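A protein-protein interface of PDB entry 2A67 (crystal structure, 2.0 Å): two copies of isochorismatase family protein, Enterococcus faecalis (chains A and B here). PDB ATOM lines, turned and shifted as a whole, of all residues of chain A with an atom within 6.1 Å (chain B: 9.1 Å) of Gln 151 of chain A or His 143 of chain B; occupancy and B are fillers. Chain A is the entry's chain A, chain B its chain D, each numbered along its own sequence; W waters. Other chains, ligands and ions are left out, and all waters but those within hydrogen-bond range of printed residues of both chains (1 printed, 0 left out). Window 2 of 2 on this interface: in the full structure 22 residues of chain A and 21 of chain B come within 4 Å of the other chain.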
ATOM      1  N   ALA A 146      -5.277 -24.913 -21.434  1.00  0.00           N
ATOM      2  CA  ALA A 146      -6.621 -24.412 -21.674  1.00  0.00           C
ATOM      3  C   ALA A 146      -6.738 -22.964 -21.206  1.00  0.00           C
ATOM      4  O   ALA A 146      -7.287 -22.147 -21.916  1.00  0.00           O
ATOM      5  CB  ALA A 146      -7.657 -25.270 -21.015  1.00  0.00           C
ATOM      6  N   ALA A 147      -6.208 -22.635 -20.026  1.00  0.00           N
ATOM      7  CA  ALA A 147      -6.334 -21.262 -19.472  1.00  0.00           C
ATOM      8  C   ALA A 147      -5.661 -20.211 -20.393  1.00  0.00           C
ATOM      9  O   ALA A 147      -6.181 -19.133 -20.601  1.00  0.00           O
ATOM     10  CB  ALA A 147      -5.717 -21.194 -17.998  1.00  0.00           C
ATOM     11  N   GLN A 148      -4.479 -20.522 -20.911  1.00  0.00           N
ATOM     12  CA  GLN A 148      -3.794 -19.613 -21.849  1.00  0.00           C
ATOM     13  C   GLN A 148      -4.618 -19.369 -23.127  1.00  0.00           C
ATOM     14  O   GLN A 148      -4.731 -18.232 -23.609  1.00  0.00           O
ATOM     15  CB  GLN A 148      -2.436 -20.202 -22.288  1.00  0.00           C
ATOM     16  CG  GLN A 148      -1.320 -20.053 -21.240  1.00  0.00           C
ATOM     17  CD  GLN A 148      -0.082 -20.734 -21.666  1.00  0.00           C
ATOM     18  OE1 GLN A 148      -0.076 -21.965 -21.828  1.00  0.00           O
ATOM     19  NE2 GLN A 148       0.988 -19.958 -21.894  1.00  0.00           N
ATOM     20  N   ILE A 149      -5.162 -20.451 -23.669  1.00  0.00           N
ATOM     21  CA  ILE A 149      -6.020 -20.373 -24.879  1.00  0.00           C
ATOM     22  C   ILE A 149      -7.256 -19.500 -24.602  1.00  0.00           C
ATOM     23  O   ILE A 149      -7.642 -18.673 -25.427  1.00  0.00           O
ATOM     24  CB  ILE A 149      -6.422 -21.778 -25.388  1.00  0.00           C
ATOM     25  CG1 ILE A 149      -5.174 -22.593 -25.792  1.00  0.00           C
ATOM     26  CG2 ILE A 149      -7.367 -21.647 -26.631  1.00  0.00           C
ATOM     27  CD1 ILE A 149      -5.403 -24.122 -25.917  1.00  0.00           C
ATOM     28  N   ILE A 150      -7.910 -19.719 -23.462  1.00  0.00           N
ATOM     29  CA  ILE A 150      -9.111 -18.936 -23.084  1.00  0.00           C
ATOM     30  C   ILE A 150      -8.735 -17.472 -22.939  1.00  0.00           C
ATOM     31  O   ILE A 150      -9.386 -16.588 -23.481  1.00  0.00           O
ATOM     32  CB  ILE A 150      -9.733 -19.490 -21.808  1.00  0.00           C
ATOM     33  CG1 ILE A 150     -10.369 -20.863 -22.086  1.00  0.00           C
ATOM     34  CG2 ILE A 150     -10.774 -18.495 -21.184  1.00  0.00           C
ATOM     35  CD1 ILE A 150     -10.534 -21.738 -20.894  1.00  0.00           C
ATOM     36  N   GLN A 151      -7.638 -17.197 -22.236  1.00  0.00           N
ATOM     37  CA  GLN A 151      -7.227 -15.809 -22.051  1.00  0.00           C
ATOM     38  C   GLN A 151      -6.961 -15.179 -23.423  1.00  0.00           C
ATOM     39  O   GLN A 151      -7.371 -14.036 -23.688  1.00  0.00           O
ATOM     40  CB  GLN A 151      -5.945 -15.749 -21.185  1.00  0.00           C
ATOM     41  CG  GLN A 151      -5.393 -14.359 -21.003  1.00  0.00           C
ATOM     42  CD  GLN A 151      -4.034 -14.353 -20.295  1.00  0.00           C
ATOM     43  OE1 GLN A 151      -3.033 -14.902 -20.788  1.00  0.00           O
ATOM     44  NE2 GLN A 151      -3.983 -13.684 -19.146  1.00  0.00           N
ATOM     45  N   HIS A 152      -6.281 -15.936 -24.301  1.00  0.00           N
ATOM     46  CA  HIS A 152      -5.904 -15.399 -25.605  1.00  0.00           C
ATOM     47  C   HIS A 152      -7.137 -15.036 -26.440  1.00  0.00           C
ATOM     48  O   HIS A 152      -7.264 -13.917 -26.924  1.00  0.00           O
ATOM     49  CB  HIS A 152      -4.960 -16.355 -26.336  1.00  0.00           C
ATOM     50  CG  HIS A 152      -4.619 -15.933 -27.724  1.00  0.00           C
ATOM     51  ND1 HIS A 152      -3.776 -14.873 -28.000  1.00  0.00           N
ATOM     52  CD2 HIS A 152      -4.969 -16.465 -28.931  1.00  0.00           C
ATOM     53  CE1 HIS A 152      -3.639 -14.754 -29.314  1.00  0.00           C
ATOM     54  NE2 HIS A 152      -4.359 -15.703 -29.900  1.00  0.00           N
ATOM     55  N   HIS A 153      -8.082 -15.961 -26.560  1.00  0.00           N
ATOM     56  CA  HIS A 153      -9.188 -15.720 -27.458  1.00  0.00           C
ATOM     57  C   HIS A 153     -10.168 -14.700 -26.900  1.00  0.00           C
ATOM     58  O   HIS A 153     -10.667 -13.867 -27.632  1.00  0.00           O
ATOM     59  CB  HIS A 153      -9.876 -17.010 -27.841  1.00  0.00           C
ATOM     60  CG  HIS A 153      -9.161 -17.718 -28.939  1.00  0.00           C
ATOM     61  ND1 HIS A 153      -8.018 -18.449 -28.717  1.00  0.00           N
ATOM     62  CD2 HIS A 153      -9.379 -17.743 -30.276  1.00  0.00           C
ATOM     63  CE1 HIS A 153      -7.571 -18.937 -29.871  1.00  0.00           C
ATOM     64  NE2 HIS A 153      -8.377 -18.515 -30.833  1.00  0.00           N
ATOM     65  N   GLU A 154     -10.478 -14.806 -25.620  1.00  0.00           N
ATOM     66  CA  GLU A 154     -11.405 -13.876 -24.995  1.00  0.00           C
ATOM     67  C   GLU A 154     -10.926 -12.416 -25.095  1.00  0.00           C
ATOM     68  O   GLU A 154     -11.726 -11.518 -25.338  1.00  0.00           O
ATOM     69  CB  GLU A 154     -11.681 -14.324 -23.555  1.00  0.00           C
ATOM     70  CG  GLU A 154     -12.524 -15.609 -23.579  1.00  0.00           C
ATOM     71  CD  GLU A 154     -13.079 -16.064 -22.239  1.00  0.00           C
ATOM     72  OE1 GLU A 154     -12.664 -15.498 -21.227  1.00  0.00           O
ATOM     73  OE2 GLU A 154     -13.901 -17.042 -22.209  1.00  0.00           O
ATOM     74  N   ALA A 155      -9.618 -12.204 -24.982  1.00  0.00           N
ATOM     75  CA  ALA A 155      -9.012 -10.882 -25.178  1.00  0.00           C
ATOM     76  C   ALA A 155      -9.147 -10.379 -26.602  1.00  0.00           C
ATOM     77  O   ALA A 155      -9.352  -9.199 -26.814  1.00  0.00           O
ATOM     78  CB  ALA A 155      -7.505 -10.874 -24.742  1.00  0.00           C
ATOM     79  N   ILE A 156      -9.018 -11.262 -27.606  1.00  0.00           N
ATOM     80  CA  ILE A 156      -9.306 -10.834 -28.959  1.00  0.00           C
ATOM     81  C   ILE A 156     -10.768 -10.401 -29.107  1.00  0.00           C
ATOM     82  O   ILE A 156     -11.067  -9.366 -29.742  1.00  0.00           O
ATOM     83  CB  ILE A 156      -8.984 -12.020 -30.031  1.00  0.00           C
ATOM     84  CG1 ILE A 156      -7.483 -12.383 -30.030  1.00  0.00           C
ATOM     85  CG2 ILE A 156      -9.477 -11.628 -31.470  1.00  0.00           C
ATOM     86  CD1 ILE A 156      -7.200 -13.779 -30.810  1.00  0.00           C
ATOM     87  N   LEU B 139       2.842  -9.597 -33.253  1.00  0.00           N
ATOM     88  CA  LEU B 139       3.663  -8.969 -32.199  1.00  0.00           C
ATOM     89  C   LEU B 139       3.567  -9.794 -30.929  1.00  0.00           C
ATOM     90  O   LEU B 139       2.543 -10.461 -30.707  1.00  0.00           O
ATOM     91  CB  LEU B 139       3.126  -7.559 -31.918  1.00  0.00           C
ATOM     92  CG  LEU B 139       2.908  -6.621 -33.117  1.00  0.00           C
ATOM     93  CD1 LEU B 139       2.049  -5.436 -32.747  1.00  0.00           C
ATOM     94  CD2 LEU B 139       4.220  -6.122 -33.709  1.00  0.00           C
ATOM     95  N   ASP B 140       4.611  -9.762 -30.086  1.00  0.00           N
ATOM     96  CA  ASP B 140       4.509 -10.348 -28.756  1.00  0.00           C
ATOM     97  C   ASP B 140       3.375  -9.548 -28.160  1.00  0.00           C
ATOM     98  O   ASP B 140       3.301  -8.346 -28.387  1.00  0.00           O
ATOM     99  CB  ASP B 140       5.783 -10.127 -27.897  1.00  0.00           C
ATOM    100  CG  ASP B 140       7.038 -10.875 -28.432  1.00  0.00           C
ATOM    101  OD1 ASP B 140       6.950 -11.774 -29.316  1.00  0.00           O
ATOM    102  OD2 ASP B 140       8.150 -10.548 -27.954  1.00  0.00           O
ATOM    103  N   ASN B 141       2.475 -10.192 -27.429  1.00  0.00           N
ATOM    104  CA  ASN B 141       1.327  -9.470 -26.882  1.00  0.00           C
ATOM    105  C   ASN B 141       1.362  -9.315 -25.363  1.00  0.00           C
ATOM    106  O   ASN B 141       0.342  -8.960 -24.764  1.00  0.00           O
ATOM    107  CB  ASN B 141      -0.014 -10.078 -27.348  1.00  0.00           C
ATOM    108  CG  ASN B 141      -0.307 -11.414 -26.725  1.00  0.00           C
ATOM    109  OD1 ASN B 141      -1.249 -12.124 -27.129  1.00  0.00           O
ATOM    110  ND2 ASN B 141       0.484 -11.791 -25.754  1.00  0.00           N
ATOM    111  N   GLY B 142       2.504  -9.593 -24.730  1.00  0.00           N
ATOM    112  CA  GLY B 142       2.596  -9.484 -23.265  1.00  0.00           C
ATOM    113  C   GLY B 142       2.135 -10.747 -22.548  1.00  0.00           C
ATOM    114  O   GLY B 142       2.377 -10.916 -21.362  1.00  0.00           O
ATOM    115  N   HIS B 143       1.452 -11.645 -23.249  1.00  0.00           N
ATOM    116  CA  HIS B 143       1.120 -12.960 -22.658  1.00  0.00           C
ATOM    117  C   HIS B 143       1.763 -14.134 -23.425  1.00  0.00           C
ATOM    118  O   HIS B 143       2.093 -15.164 -22.851  1.00  0.00           O
ATOM    119  CB  HIS B 143      -0.396 -13.161 -22.582  1.00  0.00           C
ATOM    120  CG  HIS B 143      -1.111 -12.130 -21.756  1.00  0.00           C
ATOM    121  ND1 HIS B 143      -1.411 -12.317 -20.418  1.00  0.00           N
ATOM    122  CD2 HIS B 143      -1.597 -10.907 -22.082  1.00  0.00           C
ATOM    123  CE1 HIS B 143      -2.036 -11.251 -19.953  1.00  0.00           C
ATOM    124  NE2 HIS B 143      -2.163 -10.380 -20.941  1.00  0.00           N
ATOM    125  N   LEU B 144       1.919 -13.970 -24.734  1.00  0.00           N
ATOM    126  CA  LEU B 144       2.417 -15.011 -25.610  1.00  0.00           C
ATOM    127  C   LEU B 144       3.358 -14.334 -26.581  1.00  0.00           C
ATOM    128  O   LEU B 144       3.165 -13.172 -26.903  1.00  0.00           O
ATOM    129  CB  LEU B 144       1.237 -15.612 -26.394  1.00  0.00           C
ATOM    130  CG  LEU B 144       0.541 -16.960 -26.146  1.00  0.00           C
ATOM    131  CD1 LEU B 144       0.655 -17.540 -24.774  1.00  0.00           C
ATOM    132  CD2 LEU B 144      -0.947 -16.970 -26.654  1.00  0.00           C
ATOM    133  N   THR B 145       4.393 -15.033 -27.037  1.00  0.00           N
ATOM    134  CA  THR B 145       5.288 -14.444 -28.045  1.00  0.00           C
ATOM    135  C   THR B 145       4.597 -14.520 -29.404  1.00  0.00           C
ATOM    136  O   THR B 145       3.665 -15.308 -29.562  1.00  0.00           O
ATOM    137  CB  THR B 145       6.591 -15.241 -28.169  1.00  0.00           C
ATOM    138  OG1 THR B 145       6.279 -16.612 -28.473  1.00  0.00           O
ATOM    139  CG2 THR B 145       7.408 -15.164 -26.863  1.00  0.00           C
ATOM    140  N   ALA B 146       5.070 -13.732 -30.370  1.00  0.00           N
ATOM    141  CA  ALA B 146       4.617 -13.814 -31.765  1.00  0.00           C
ATOM    142  C   ALA B 146       4.714 -15.233 -32.287  1.00  0.00           C
ATOM    143  O   ALA B 146       3.774 -15.713 -32.907  1.00  0.00           O
ATOM    144  CB  ALA B 146       5.425 -12.910 -32.642  1.00  0.00           C
ATOM    145  N   GLN B 148       4.515 -18.109 -30.629  1.00  0.00           N
ATOM    146  CA  GLN B 148       3.483 -18.967 -30.036  1.00  0.00           C
ATOM    147  C   GLN B 148       2.108 -18.688 -30.636  1.00  0.00           C
ATOM    148  O   GLN B 148       1.310 -19.624 -30.868  1.00  0.00           O
ATOM    149  CB  GLN B 148       3.393 -18.716 -28.522  1.00  0.00           C
ATOM    150  CG  GLN B 148       4.564 -19.198 -27.688  1.00  0.00           C
ATOM    151  CD  GLN B 148       4.352 -18.868 -26.231  1.00  0.00           C
ATOM    152  OE1 GLN B 148       4.362 -17.701 -25.849  1.00  0.00           O
ATOM    153  NE2 GLN B 148       4.114 -19.878 -25.420  1.00  0.00           N
ATOM    154  N   ILE B 149       1.829 -17.401 -30.862  1.00  0.00           N
ATOM    155  CA  ILE B 149       0.571 -16.948 -31.499  1.00  0.00           C
ATOM    156  C   ILE B 149       0.450 -17.480 -32.927  1.00  0.00           C
ATOM    157  O   ILE B 149      -0.610 -17.995 -33.318  1.00  0.00           O
ATOM    158  CB  ILE B 149       0.410 -15.404 -31.517  1.00  0.00           C
ATOM    159  CG1 ILE B 149       0.385 -14.828 -30.083  1.00  0.00           C
ATOM    160  CG2 ILE B 149      -0.897 -15.004 -32.324  1.00  0.00           C
ATOM    161  CD1 ILE B 149       0.689 -13.322 -30.047  1.00  0.00           C
ATOM    162  N   HIS B 152      -0.039 -21.303 -32.860  1.00  0.00           N
ATOM    163  CA  HIS B 152      -1.409 -21.570 -32.446  1.00  0.00           C
ATOM    164  C   HIS B 152      -2.426 -21.407 -33.583  1.00  0.00           C
ATOM    165  O   HIS B 152      -3.211 -22.301 -33.802  1.00  0.00           O
ATOM    166  CB  HIS B 152      -1.786 -20.640 -31.277  1.00  0.00           C
ATOM    167  CG  HIS B 152      -3.187 -20.817 -30.760  1.00  0.00           C
ATOM    168  ND1 HIS B 152      -3.640 -21.992 -30.190  1.00  0.00           N
ATOM    169  CD2 HIS B 152      -4.215 -19.932 -30.674  1.00  0.00           C
ATOM    170  CE1 HIS B 152      -4.879 -21.810 -29.746  1.00  0.00           C
ATOM    171  NE2 HIS B 152      -5.255 -20.575 -30.051  1.00  0.00           N
HETATM  172  O   HOH W   1      -2.508 -13.874 -25.627  1.00  0.00           O
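A ring nitrogen (ND1) of His 143 of chain B sits at hydrogen-bond distance from the side-chain amide oxygen (OE1) of Gln 151 of chain A (3.1 Å).
The backbone carbonyl oxygen (O) of Ile 149 of chain A is in hydrogen-bond range of a ring nitrogen (ND1) of His 153 of chain A (3.3 Å).
ND2 of Asn 141 of chain B lies close to N of His 143 of chain B.
The side-chain amide nitrogen (ND2) of Asn 141 of chain B lies close to the backbone NH (N) of Leu 144 of chain B (2.8 Å).
Among the printed residues, pairs that only touch across the chains: His 153 of chain A with His 152 of chain B (2.8 Å), His 152 of chain A with Leu 144 of chain B (3.8 Å), Gln 148 of chain A with Leu 144 of chain B (3.8 Å), His 152 of chain A with Asn 141 of chain B (3.8 Å), His 152 of chain A with His 152 of chain B (3.95 Å) and Ile 149 of chain A with His 152 of chain B (3.99 Å).
Of the printed residues of chain B, Ile 149 of chain A touches His 152.
Of the printed residues of chain B, His 153 of chain A touches His 152.
Of the printed residues of chain A, Asn 141 of chain B touches His 152.
Gln 148 of chain B touches none of the printed residues of chain A.
The nearest residue of chain A that does not touch His 143 of chain B is Gln 148 of chain A (5.0 Å).
Of the 11 printed residues of chain B, 4 touch a printed residue of chain A.
Hydrophobic or aromatic side chains of chain B that line the printed part of chain A: His 143, Leu 144 and His 152.
Hydrophobic or aromatic side chains of chain A within 4 Å of the printed part of chain B: Ile 149, His 152 and His 153.
Among the printed residues, no Asp or Glu carboxylate lies within 4 Å of a Lys or Arg side-chain nitrogen of the other chain.
Ile 149 of chain A touches His 152 of chain B, but with the chains exchanged His 152 of chain A does not touch Ile 149 of chain B (4.1 Å).
His 152 of chain A touches its own counterpart, His 152 of chain B.
Positions printed for both chains: 146, 148, 149 and 152.
Of the 7 pairs that touch across the chains among the printed residues, 1 has its exchanged pair printed and touching as well.
Water W1 lies within hydrogen-bond range of the side-chain amide oxygen (OD1) of Asn 141 of chain B (2.6 Å) and a ring nitrogen (ND1) of His 152 of chain A (2.9 Å).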
